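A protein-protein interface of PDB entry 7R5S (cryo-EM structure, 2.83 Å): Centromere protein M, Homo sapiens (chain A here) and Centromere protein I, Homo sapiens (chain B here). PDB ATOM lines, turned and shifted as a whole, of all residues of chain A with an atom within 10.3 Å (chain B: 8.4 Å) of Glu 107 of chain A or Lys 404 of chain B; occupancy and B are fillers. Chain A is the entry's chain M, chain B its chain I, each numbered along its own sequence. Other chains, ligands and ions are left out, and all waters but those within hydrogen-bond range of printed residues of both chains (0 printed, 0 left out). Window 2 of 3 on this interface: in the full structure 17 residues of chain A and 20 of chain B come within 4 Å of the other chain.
Of the 18 printed residues of chain A, 3 touch a printed residue of chain B.
The backbone carbonyl oxygen (O) of Gly 105 of chain A sits at hydrogen-bond distance from the backbone NH (N) of Val 405 of chain B (3.4 Å). The side-chain carboxylate (OD2) of Asp 132 of chain A lies close to the side-chain amide oxygen (OD1) of Asn 406 of chain B, at 3.4 Å.
OH of Tyr 403 of chain B sits at hydrogen-bond distance from NZ of Lys 404 of chain B (2.6 Å). N of Gly 103 of chain A lies within hydrogen-bond range of OD1 of Asp 132 of chain A (3.4 Å).
Among the printed residues, pairs that only touch across the chains: Gly 105 of chain A with Lys 404 of chain B (3.3 Å) and Glu 107 of chain A with Lys 404 of chain B (3.9 Å).
Of the printed residues of chain B, Gly 105 of chain A touches Lys 404 and Val 405. Printed residues of chain B within 4 Å of Glu 107 of chain A: Lys 404 (3.9 Å). Ile 112 of chain A touches none of the printed residues of chain B. Of the printed residues of chain B, Asp 132 of chain A touches Asn 406 (3.4 Å). Gln 397 of chain B touches none of the printed residues of chain A. Tyr 403 of chain B touches none of the printed residues of chain A. Printed residues of chain A within 4 Å of Lys 404 of chain B: Gly 105 and Glu 107. Val 405 of chain B touches just one residue of chain A: Gly 105 (3.4 Å). Printed residues of chain A within 4 Å of Asn 406 of chain B: Asp 132 (3.4 Å). The nearest printed residue of chain B that does not touch Asp 132 of chain A is Trp 402 of chain B (5.3 Å).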
ATOM      1  N   LEU A  72      28.195 -19.621  21.214  1.00  0.00           N
ATOM      2  CA  LEU A  72      29.173 -20.700  21.281  1.00  0.00           C
ATOM      3  C   LEU A  72      29.250 -21.520  20.000  1.00  0.00           C
ATOM      4  O   LEU A  72      30.080 -22.433  19.926  1.00  0.00           O
ATOM      5  CB  LEU A  72      28.857 -21.620  22.460  1.00  0.00           C
ATOM      6  CG  LEU A  72      28.920 -20.995  23.854  1.00  0.00           C
ATOM      7  CD1 LEU A  72      28.574 -22.022  24.918  1.00  0.00           C
ATOM      8  CD2 LEU A  72      30.293 -20.397  24.112  1.00  0.00           C
ATOM      9  N   HIS A  73      28.420 -21.231  19.001  1.00  0.00           N
ATOM     10  CA  HIS A  73      28.415 -21.971  17.748  1.00  0.00           C
ATOM     11  C   HIS A  73      29.214 -21.280  16.650  1.00  0.00           C
ATOM     12  O   HIS A  73      29.225 -21.761  15.512  1.00  0.00           O
ATOM     13  CB  HIS A  73      26.978 -22.200  17.277  1.00  0.00           C
ATOM     14  CG  HIS A  73      26.164 -23.046  18.205  1.00  0.00           C
ATOM     15  ND1 HIS A  73      24.813 -23.255  18.030  1.00  0.00           N
ATOM     16  CD2 HIS A  73      26.509 -23.738  19.317  1.00  0.00           C
ATOM     17  CE1 HIS A  73      24.360 -24.038  18.993  1.00  0.00           C
ATOM     18  NE2 HIS A  73      25.370 -24.345  19.787  1.00  0.00           N
ATOM     19  N   THR A 102      25.260 -18.149  24.707  1.00  0.00           N
ATOM     20  CA  THR A 102      24.117 -18.775  24.061  1.00  0.00           C
ATOM     21  C   THR A 102      24.568 -19.999  23.277  1.00  0.00           C
ATOM     22  O   THR A 102      25.584 -19.959  22.575  1.00  0.00           O
ATOM     23  CB  THR A 102      23.405 -17.792  23.123  1.00  0.00           C
ATOM     24  OG1 THR A 102      23.092 -16.591  23.837  1.00  0.00           O
ATOM     25  CG2 THR A 102      22.121 -18.399  22.583  1.00  0.00           C
ATOM     26  N   GLY A 103      23.810 -21.086  23.399  1.00  0.00           N
ATOM     27  CA  GLY A 103      24.065 -22.295  22.646  1.00  0.00           C
ATOM     28  C   GLY A 103      24.673 -23.445  23.418  1.00  0.00           C
ATOM     29  O   GLY A 103      25.095 -24.426  22.796  1.00  0.00           O
ATOM     30  N   ALA A 104      24.731 -23.366  24.749  1.00  0.00           N
ATOM     31  CA  ALA A 104      25.311 -24.445  25.538  1.00  0.00           C
ATOM     32  C   ALA A 104      24.400 -25.661  25.641  1.00  0.00           C
ATOM     33  O   ALA A 104      24.850 -26.710  26.113  1.00  0.00           O
ATOM     34  CB  ALA A 104      25.661 -23.943  26.939  1.00  0.00           C
ATOM     35  N   GLY A 105      23.140 -25.548  25.217  1.00  0.00           N
ATOM     36  CA  GLY A 105      22.243 -26.692  25.292  1.00  0.00           C
ATOM     37  C   GLY A 105      22.591 -27.769  24.281  1.00  0.00           C
ATOM     38  O   GLY A 105      22.651 -28.955  24.616  1.00  0.00           O
ATOM     39  N   ARG A 106      22.823 -27.370  23.031  1.00  0.00           N
ATOM     40  CA  ARG A 106      23.196 -28.302  21.968  1.00  0.00           C
ATOM     41  C   ARG A 106      24.716 -28.390  21.932  1.00  0.00           C
ATOM     42  O   ARG A 106      25.394 -27.580  21.300  1.00  0.00           O
ATOM     43  CB  ARG A 106      22.621 -27.854  20.631  1.00  0.00           C
ATOM     44  CG  ARG A 106      21.105 -27.912  20.562  1.00  0.00           C
ATOM     45  CD  ARG A 106      20.589 -27.421  19.221  1.00  0.00           C
ATOM     46  NE  ARG A 106      20.849 -25.998  19.023  1.00  0.00           N
ATOM     47  CZ  ARG A 106      20.458 -25.311  17.956  1.00  0.00           C
ATOM     48  NH1 ARG A 106      19.787 -25.914  16.984  1.00  0.00           N
ATOM     49  NH2 ARG A 106      20.738 -24.018  17.857  1.00  0.00           N
ATOM     50  N   GLU A 107      25.258 -29.395  22.624  1.00  0.00           N
ATOM     51  CA  GLU A 107      26.708 -29.535  22.713  1.00  0.00           C
ATOM     52  C   GLU A 107      27.317 -29.989  21.392  1.00  0.00           C
ATOM     53  O   GLU A 107      28.484 -29.688  21.114  1.00  0.00           O
ATOM     54  CB  GLU A 107      27.070 -30.512  23.831  1.00  0.00           C
ATOM     55  CG  GLU A 107      28.552 -30.555  24.167  1.00  0.00           C
ATOM     56  CD  GLU A 107      28.871 -31.538  25.275  1.00  0.00           C
ATOM     57  OE1 GLU A 107      30.067 -31.824  25.492  1.00  0.00           O
ATOM     58  OE2 GLU A 107      27.925 -32.024  25.931  1.00  0.00           O
ATOM     59  N   SER A 108      26.550 -30.704  20.567  1.00  0.00           N
ATOM     60  CA  SER A 108      27.072 -31.187  19.294  1.00  0.00           C
ATOM     61  C   SER A 108      27.360 -30.057  18.315  1.00  0.00           C
ATOM     62  O   SER A 108      28.165 -30.242  17.396  1.00  0.00           O
ATOM     63  CB  SER A 108      26.091 -32.179  18.668  1.00  0.00           C
ATOM     64  OG  SER A 108      24.759 -31.702  18.754  1.00  0.00           O
ATOM     65  N   HIS A 109      26.727 -28.898  18.487  1.00  0.00           N
ATOM     66  CA  HIS A 109      26.939 -27.759  17.605  1.00  0.00           C
ATOM     67  C   HIS A 109      28.015 -26.805  18.107  1.00  0.00           C
ATOM     68  O   HIS A 109      28.454 -25.938  17.343  1.00  0.00           O
ATOM     69  CB  HIS A 109      25.633 -26.980  17.421  1.00  0.00           C
ATOM     70  CG  HIS A 109      24.574 -27.731  16.675  1.00  0.00           C
ATOM     71  ND1 HIS A 109      24.144 -28.985  17.051  1.00  0.00           N
ATOM     72  CD2 HIS A 109      23.852 -27.400  15.579  1.00  0.00           C
ATOM     73  CE1 HIS A 109      23.207 -29.396  16.215  1.00  0.00           C
ATOM     74  NE2 HIS A 109      23.012 -28.452  15.313  1.00  0.00           N
ATOM     75  N   CYS A 110      28.447 -26.941  19.358  1.00  0.00           N
ATOM     76  CA  CYS A 110      29.372 -25.983  19.945  1.00  0.00           C
ATOM     77  C   CYS A 110      30.751 -26.093  19.307  1.00  0.00           C
ATOM     78  O   CYS A 110      31.299 -27.191  19.169  1.00  0.00           O
ATOM     79  CB  CYS A 110      29.472 -26.198  21.454  1.00  0.00           C
ATOM     80  SG  CYS A 110      27.947 -25.866  22.360  1.00  0.00           S
ATOM     81  N   SER A 111      31.309 -24.950  18.919  1.00  0.00           N
ATOM     82  CA  SER A 111      32.662 -24.870  18.390  1.00  0.00           C
ATOM     83  C   SER A 111      33.637 -24.228  19.367  1.00  0.00           C
ATOM     84  O   SER A 111      34.838 -24.184  19.086  1.00  0.00           O
ATOM     85  CB  SER A 111      32.666 -24.090  17.071  1.00  0.00           C
ATOM     86  OG  SER A 111      33.985 -23.741  16.692  1.00  0.00           O
ATOM     87  N   ILE A 112      33.150 -23.733  20.502  1.00  0.00           N
ATOM     88  CA  ILE A 112      33.972 -23.065  21.504  1.00  0.00           C
ATOM     89  C   ILE A 112      33.798 -23.795  22.828  1.00  0.00           C
ATOM     90  O   ILE A 112      32.668 -24.083  23.238  1.00  0.00           O
ATOM     91  CB  ILE A 112      33.595 -21.579  21.646  1.00  0.00           C
ATOM     92  CG1 ILE A 112      33.697 -20.870  20.295  1.00  0.00           C
ATOM     93  CG2 ILE A 112      34.482 -20.897  22.675  1.00  0.00           C
ATOM     94  CD1 ILE A 112      33.261 -19.424  20.333  1.00  0.00           C
ATOM     95  N   HIS A 113      34.912 -24.093  23.488  1.00  0.00           N
ATOM     96  CA  HIS A 113      34.862 -24.747  24.787  1.00  0.00           C
ATOM     97  C   HIS A 113      34.342 -23.784  25.849  1.00  0.00           C
ATOM     98  O   HIS A 113      34.539 -22.568  25.770  1.00  0.00           O
ATOM     99  CB  HIS A 113      36.248 -25.261  25.177  1.00  0.00           C
ATOM    100  CG  HIS A 113      36.219 -26.498  26.019  1.00  0.00           C
ATOM    101  ND1 HIS A 113      36.232 -26.462  27.397  1.00  0.00           N
ATOM    102  CD2 HIS A 113      36.184 -27.808  25.679  1.00  0.00           C
ATOM    103  CE1 HIS A 113      36.203 -27.695  27.868  1.00  0.00           C
ATOM    104  NE2 HIS A 113      36.174 -28.531  26.846  1.00  0.00           N
ATOM    105  N   ARG A 114      33.663 -24.344  26.854  1.00  0.00           N
ATOM    106  CA  ARG A 114      33.120 -23.515  27.926  1.00  0.00           C
ATOM    107  C   ARG A 114      34.221 -22.944  28.812  1.00  0.00           C
ATOM    108  O   ARG A 114      34.030 -21.891  29.435  1.00  0.00           O
ATOM    109  CB  ARG A 114      32.128 -24.322  28.764  1.00  0.00           C
ATOM    110  CG  ARG A 114      30.841 -24.666  28.032  1.00  0.00           C
ATOM    111  CD  ARG A 114      29.976 -25.616  28.841  1.00  0.00           C
ATOM    112  NE  ARG A 114      29.739 -25.125  30.195  1.00  0.00           N
ATOM    113  CZ  ARG A 114      28.985 -25.750  31.093  1.00  0.00           C
ATOM    114  NH1 ARG A 114      28.391 -26.893  30.782  1.00  0.00           N
ATOM    115  NH2 ARG A 114      28.825 -25.231  32.302  1.00  0.00           N
ATOM    116  N   ASP A 132      19.494 -20.300  26.290  1.00  0.00           N
ATOM    117  CA  ASP A 132      19.256 -20.626  24.885  1.00  0.00           C
ATOM    118  C   ASP A 132      18.198 -19.660  24.366  1.00  0.00           C
ATOM    119  O   ASP A 132      17.004 -19.833  24.623  1.00  0.00           O
ATOM    120  CB  ASP A 132      18.822 -22.078  24.726  1.00  0.00           C
ATOM    121  CG  ASP A 132      19.965 -23.054  24.921  1.00  0.00           C
ATOM    122  OD1 ASP A 132      21.107 -22.716  24.549  1.00  0.00           O
ATOM    123  OD2 ASP A 132      19.721 -24.161  25.446  1.00  0.00           O
ATOM    124  N   GLU A 134      16.922 -19.238  21.564  1.00  0.00           N
ATOM    125  CA  GLU A 134      15.988 -19.731  20.560  1.00  0.00           C
ATOM    126  C   GLU A 134      14.657 -20.166  21.157  1.00  0.00           C
ATOM    127  O   GLU A 134      13.654 -20.204  20.436  1.00  0.00           O
ATOM    128  CB  GLU A 134      16.609 -20.896  19.783  1.00  0.00           C
ATOM    129  CG  GLU A 134      17.307 -21.928  20.652  1.00  0.00           C
ATOM    130  CD  GLU A 134      18.804 -21.700  20.741  1.00  0.00           C
ATOM    131  OE1 GLU A 134      19.551 -22.692  20.868  1.00  0.00           O
ATOM    132  OE2 GLU A 134      19.234 -20.528  20.680  1.00  0.00           O
ATOM    133  N   PHE A 138      12.633 -19.845  28.129  1.00  0.00           N
ATOM    134  CA  PHE A 138      13.837 -19.434  28.841  1.00  0.00           C
ATOM    135  C   PHE A 138      14.180 -17.975  28.572  1.00  0.00           C
ATOM    136  O   PHE A 138      14.720 -17.292  29.454  1.00  0.00           O
ATOM    137  CB  PHE A 138      15.014 -20.327  28.446  1.00  0.00           C
ATOM    138  CG  PHE A 138      14.738 -21.799  28.584  1.00  0.00           C
ATOM    139  CD1 PHE A 138      13.937 -22.277  29.607  1.00  0.00           C
ATOM    140  CD2 PHE A 138      15.282 -22.704  27.690  1.00  0.00           C
ATOM    141  CE1 PHE A 138      13.683 -23.631  29.734  1.00  0.00           C
ATOM    142  CE2 PHE A 138      15.033 -24.058  27.811  1.00  0.00           C
ATOM    143  CZ  PHE A 138      14.233 -24.520  28.834  1.00  0.00           C
ATOM    144  N   GLN B 394      22.590 -42.417  33.649  1.00  0.00           N
ATOM    145  CA  GLN B 394      22.305 -42.389  32.218  1.00  0.00           C
ATOM    146  C   GLN B 394      20.876 -41.929  31.948  1.00  0.00           C
ATOM    147  O   GLN B 394      20.635 -41.139  31.027  1.00  0.00           O
ATOM    148  CB  GLN B 394      22.555 -43.765  31.602  1.00  0.00           C
ATOM    149  CG  GLN B 394      24.016 -44.182  31.597  1.00  0.00           C
ATOM    150  CD  GLN B 394      24.884 -43.266  30.755  1.00  0.00           C
ATOM    151  OE1 GLN B 394      26.020 -42.964  31.117  1.00  0.00           O
ATOM    152  NE2 GLN B 394      24.352 -42.821  29.624  1.00  0.00           N
ATOM    153  N   LEU B 396      18.883 -39.983  33.863  1.00  0.00           N
ATOM    154  CA  LEU B 396      18.742 -38.558  34.144  1.00  0.00           C
ATOM    155  C   LEU B 396      19.444 -37.714  33.089  1.00  0.00           C
ATOM    156  O   LEU B 396      18.973 -36.625  32.740  1.00  0.00           O
ATOM    157  CB  LEU B 396      19.289 -38.239  35.535  1.00  0.00           C
ATOM    158  CG  LEU B 396      18.414 -38.625  36.727  1.00  0.00           C
ATOM    159  CD1 LEU B 396      19.147 -38.366  38.032  1.00  0.00           C
ATOM    160  CD2 LEU B 396      17.101 -37.865  36.690  1.00  0.00           C
ATOM    161  N   GLN B 397      20.575 -38.198  32.568  1.00  0.00           N
ATOM    162  CA  GLN B 397      21.290 -37.445  31.544  1.00  0.00           C
ATOM    163  C   GLN B 397      20.524 -37.435  30.227  1.00  0.00           C
ATOM    164  O   GLN B 397      20.516 -36.423  29.516  1.00  0.00           O
ATOM    165  CB  GLN B 397      22.688 -38.032  31.353  1.00  0.00           C
ATOM    166  CG  GLN B 397      23.534 -37.324  30.311  1.00  0.00           C
ATOM    167  CD  GLN B 397      24.919 -37.926  30.190  1.00  0.00           C
ATOM    168  OE1 GLN B 397      25.555 -37.844  29.139  1.00  0.00           O
ATOM    169  NE2 GLN B 397      25.396 -38.536  31.268  1.00  0.00           N
ATOM    170  N   GLU B 398      19.866 -38.546  29.888  1.00  0.00           N
ATOM    171  CA  GLU B 398      19.174 -38.623  28.606  1.00  0.00           C
ATOM    172  C   GLU B 398      17.783 -38.000  28.648  1.00  0.00           C
ATOM    173  O   GLU B 398      17.286 -37.544  27.613  1.00  0.00           O
ATOM    174  CB  GLU B 398      19.079 -40.079  28.147  1.00  0.00           C
ATOM    175  CG  GLU B 398      20.423 -40.723  27.844  1.00  0.00           C
ATOM    176  CD  GLU B 398      21.144 -40.059  26.687  1.00  0.00           C
ATOM    177  OE1 GLU B 398      20.464 -39.567  25.762  1.00  0.00           O
ATOM    178  OE2 GLU B 398      22.393 -40.025  26.704  1.00  0.00           O
ATOM    179  N   GLU B 399      17.142 -37.969  29.814  1.00  0.00           N
ATOM    180  CA  GLU B 399      15.763 -37.508  29.917  1.00  0.00           C
ATOM    181  C   GLU B 399      15.637 -36.042  30.314  1.00  0.00           C
ATOM    182  O   GLU B 399      14.514 -35.533  30.383  1.00  0.00           O
ATOM    183  CB  GLU B 399      14.994 -38.375  30.920  1.00  0.00           C
ATOM    184  CG  GLU B 399      14.799 -39.815  30.474  1.00  0.00           C
ATOM    185  CD  GLU B 399      13.858 -39.938  29.293  1.00  0.00           C
ATOM    186  OE1 GLU B 399      12.953 -39.088  29.161  1.00  0.00           O
ATOM    187  OE2 GLU B 399      14.022 -40.885  28.496  1.00  0.00           O
ATOM    188  N   CYS B 400      16.745 -35.353  30.576  1.00  0.00           N
ATOM    189  CA  CYS B 400      16.668 -33.960  30.991  1.00  0.00           C
ATOM    190  C   CYS B 400      16.194 -33.078  29.837  1.00  0.00           C
ATOM    191  O   CYS B 400      16.326 -33.419  28.658  1.00  0.00           O
ATOM    192  CB  CYS B 400      18.021 -33.473  31.505  1.00  0.00           C
ATOM    193  SG  CYS B 400      17.979 -31.823  32.241  1.00  0.00           S
ATOM    194  N   ILE B 401      15.639 -31.921  30.195  1.00  0.00           N
ATOM    195  CA  ILE B 401      15.028 -31.029  29.218  1.00  0.00           C
ATOM    196  C   ILE B 401      15.958 -29.905  28.765  1.00  0.00           C
ATOM    197  O   ILE B 401      15.826 -29.433  27.625  1.00  0.00           O
ATOM    198  CB  ILE B 401      13.717 -30.436  29.775  1.00  0.00           C
ATOM    199  CG1 ILE B 401      12.922 -31.511  30.517  1.00  0.00           C
ATOM    200  CG2 ILE B 401      12.875 -29.839  28.657  1.00  0.00           C
ATOM    201  CD1 ILE B 401      11.633 -31.006  31.123  1.00  0.00           C
ATOM    202  N   TRP B 402      16.894 -29.472  29.608  1.00  0.00           N
ATOM    203  CA  TRP B 402      17.765 -28.348  29.286  1.00  0.00           C
ATOM    204  C   TRP B 402      19.243 -28.714  29.311  1.00  0.00           C
ATOM    205  O   TRP B 402      20.091 -27.819  29.208  1.00  0.00           O
ATOM    206  CB  TRP B 402      17.504 -27.185  30.250  1.00  0.00           C
ATOM    207  CG  TRP B 402      17.955 -27.459  31.655  1.00  0.00           C
ATOM    208  CD1 TRP B 402      19.194 -27.229  32.178  1.00  0.00           C
ATOM    209  CD2 TRP B 402      17.171 -28.016  32.715  1.00  0.00           C
ATOM    210  NE1 TRP B 402      19.231 -27.609  33.497  1.00  0.00           N
ATOM    211  CE2 TRP B 402      18.000 -28.095  33.851  1.00  0.00           C
ATOM    212  CE3 TRP B 402      15.848 -28.456  32.816  1.00  0.00           C
ATOM    213  CZ2 TRP B 402      17.550 -28.595  35.071  1.00  0.00           C
ATOM    214  CZ3 TRP B 402      15.403 -28.953  34.026  1.00  0.00           C
ATOM    215  CH2 TRP B 402      16.252 -29.018  35.137  1.00  0.00           C
ATOM    216  N   TYR B 403      19.579 -29.995  29.439  1.00  0.00           N
ATOM    217  CA  TYR B 403      20.963 -30.434  29.559  1.00  0.00           C
ATOM    218  C   TYR B 403      21.280 -31.417  28.442  1.00  0.00           C
ATOM    219  O   TYR B 403      20.595 -32.436  28.295  1.00  0.00           O
ATOM    220  CB  TYR B 403      21.219 -31.072  30.926  1.00  0.00           C
ATOM    221  CG  TYR B 403      22.641 -31.542  31.124  1.00  0.00           C
ATOM    222  CD1 TYR B 403      23.687 -30.634  31.202  1.00  0.00           C
ATOM    223  CD2 TYR B 403      22.936 -32.893  31.232  1.00  0.00           C
ATOM    224  CE1 TYR B 403      24.988 -31.059  31.381  1.00  0.00           C
ATOM    225  CE2 TYR B 403      24.235 -33.329  31.413  1.00  0.00           C
ATOM    226  CZ  TYR B 403      25.257 -32.407  31.487  1.00  0.00           C
ATOM    227  OH  TYR B 403      26.551 -32.835  31.666  1.00  0.00           O
ATOM    228  N   LYS B 404      22.304 -31.098  27.651  1.00  0.00           N
ATOM    229  CA  LYS B 404      22.866 -31.914  26.577  1.00  0.00           C
ATOM    230  C   LYS B 404      21.932 -32.075  25.384  1.00  0.00           C
ATOM    231  O   LYS B 404      22.341 -32.671  24.380  1.00  0.00           O
ATOM    232  CB  LYS B 404      23.289 -33.309  27.060  1.00  0.00           C
ATOM    233  CG  LYS B 404      24.695 -33.366  27.632  1.00  0.00           C
ATOM    234  CD  LYS B 404      25.112 -34.795  27.937  1.00  0.00           C
ATOM    235  CE  LYS B 404      26.604 -34.887  28.215  1.00  0.00           C
ATOM    236  NZ  LYS B 404      27.012 -34.031  29.362  1.00  0.00           N
ATOM    237  N   VAL B 405      20.705 -31.558  25.445  1.00  0.00           N
ATOM    238  CA  VAL B 405      19.765 -31.672  24.337  1.00  0.00           C
ATOM    239  C   VAL B 405      18.623 -30.685  24.544  1.00  0.00           C
ATOM    240  O   VAL B 405      18.262 -30.362  25.682  1.00  0.00           O
ATOM    241  CB  VAL B 405      19.241 -33.115  24.193  1.00  0.00           C
ATOM    242  CG1 VAL B 405      18.330 -33.483  25.357  1.00  0.00           C
ATOM    243  CG2 VAL B 405      18.532 -33.307  22.857  1.00  0.00           C
ATOM    244  N   ASN B 406      18.061 -30.184  23.448  1.00  0.00           N
ATOM    245  CA  ASN B 406      16.891 -29.311  23.475  1.00  0.00           C
ATOM    246  C   ASN B 406      15.691 -30.156  23.055  1.00  0.00           C
ATOM    247  O   ASN B 406      15.301 -30.172  21.886  1.00  0.00           O
ATOM    248  CB  ASN B 406      17.082 -28.103  22.559  1.00  0.00           C
ATOM    249  CG  ASN B 406      17.582 -26.881  23.302  1.00  0.00           C
ATOM    250  OD1 ASN B 406      18.032 -26.975  24.443  1.00  0.00           O
ATOM    251  ND2 ASN B 406      17.508 -25.724  22.655  1.00  0.00           N
ATOM    252  N   ASN B 407      15.106 -30.862  24.024  1.00  0.00           N
ATOM    253  CA  ASN B 407      13.989 -31.777  23.780  1.00  0.00           C
ATOM    254  C   ASN B 407      12.917 -31.521  24.834  1.00  0.00           C
ATOM    255  O   ASN B 407      12.929 -32.128  25.907  1.00  0.00           O
ATOM    256  CB  ASN B 407      14.461 -33.229  23.795  1.00  0.00           C
ATOM    257  N   PHE B 438      23.953 -35.248  38.977  1.00  0.00           N
ATOM    258  CA  PHE B 438      23.104 -34.515  38.042  1.00  0.00           C
ATOM    259  C   PHE B 438      22.902 -33.074  38.493  1.00  0.00           C
ATOM    260  O   PHE B 438      22.881 -32.154  37.668  1.00  0.00           O
ATOM    261  CB  PHE B 438      21.762 -35.231  37.888  1.00  0.00           C
ATOM    262  CG  PHE B 438      20.763 -34.476  37.061  1.00  0.00           C
ATOM    263  CD1 PHE B 438      20.894 -34.409  35.685  1.00  0.00           C
ATOM    264  CD2 PHE B 438      19.688 -33.840  37.659  1.00  0.00           C
ATOM    265  CE1 PHE B 438      19.975 -33.718  34.920  1.00  0.00           C
ATOM    266  CE2 PHE B 438      18.766 -33.148  36.899  1.00  0.00           C
ATOM    267  CZ  PHE B 438      18.909 -33.088  35.529  1.00  0.00           C
ATOM    268  N   LYS B 441      26.005 -31.155  37.729  1.00  0.00           N
ATOM    269  CA  LYS B 441      26.226 -30.966  36.298  1.00  0.00           C
ATOM    270  C   LYS B 441      25.276 -29.932  35.703  1.00  0.00           C
ATOM    271  O   LYS B 441      25.704 -29.041  34.961  1.00  0.00           O
ATOM    272  CB  LYS B 441      26.078 -32.300  35.563  1.00  0.00           C
ATOM    273  CG  LYS B 441      27.255 -33.243  35.726  1.00  0.00           C
ATOM    274  CD  LYS B 441      27.034 -34.524  34.940  1.00  0.00           C
ATOM    275  CE  LYS B 441      28.220 -35.463  35.059  1.00  0.00           C
ATOM    276  NZ  LYS B 441      28.012 -36.721  34.292  1.00  0.00           N
ATOM    277  N   SER B 442      23.984 -30.032  36.012  1.00  0.00           N
ATOM    278  CA  SER B 442      22.958 -29.262  35.318  1.00  0.00           C
ATOM    279  C   SER B 442      22.557 -27.981  36.037  1.00  0.00           C
ATOM    280  O   SER B 442      21.644 -27.293  35.574  1.00  0.00           O
ATOM    281  CB  SER B 442      21.716 -30.131  35.096  1.00  0.00           C
ATOM    282  OG  SER B 442      21.225 -30.637  36.324  1.00  0.00           O
ATOM    283  N   LEU B 445      23.298 -24.435  34.144  1.00  0.00           N
ATOM    284  CA  LEU B 445      22.478 -24.221  32.960  1.00  0.00           C
ATOM    285  C   LEU B 445      20.998 -24.052  33.281  1.00  0.00           C
ATOM    286  O   LEU B 445      20.207 -23.795  32.368  1.00  0.00           O
ATOM    287  CB  LEU B 445      22.662 -25.381  31.977  1.00  0.00           C
ATOM    288  CG  LEU B 445      24.097 -25.664  31.530  1.00  0.00           C
ATOM    289  CD1 LEU B 445      24.139 -26.850  30.582  1.00  0.00           C
ATOM    290  CD2 LEU B 445      24.711 -24.435  30.882  1.00  0.00           C
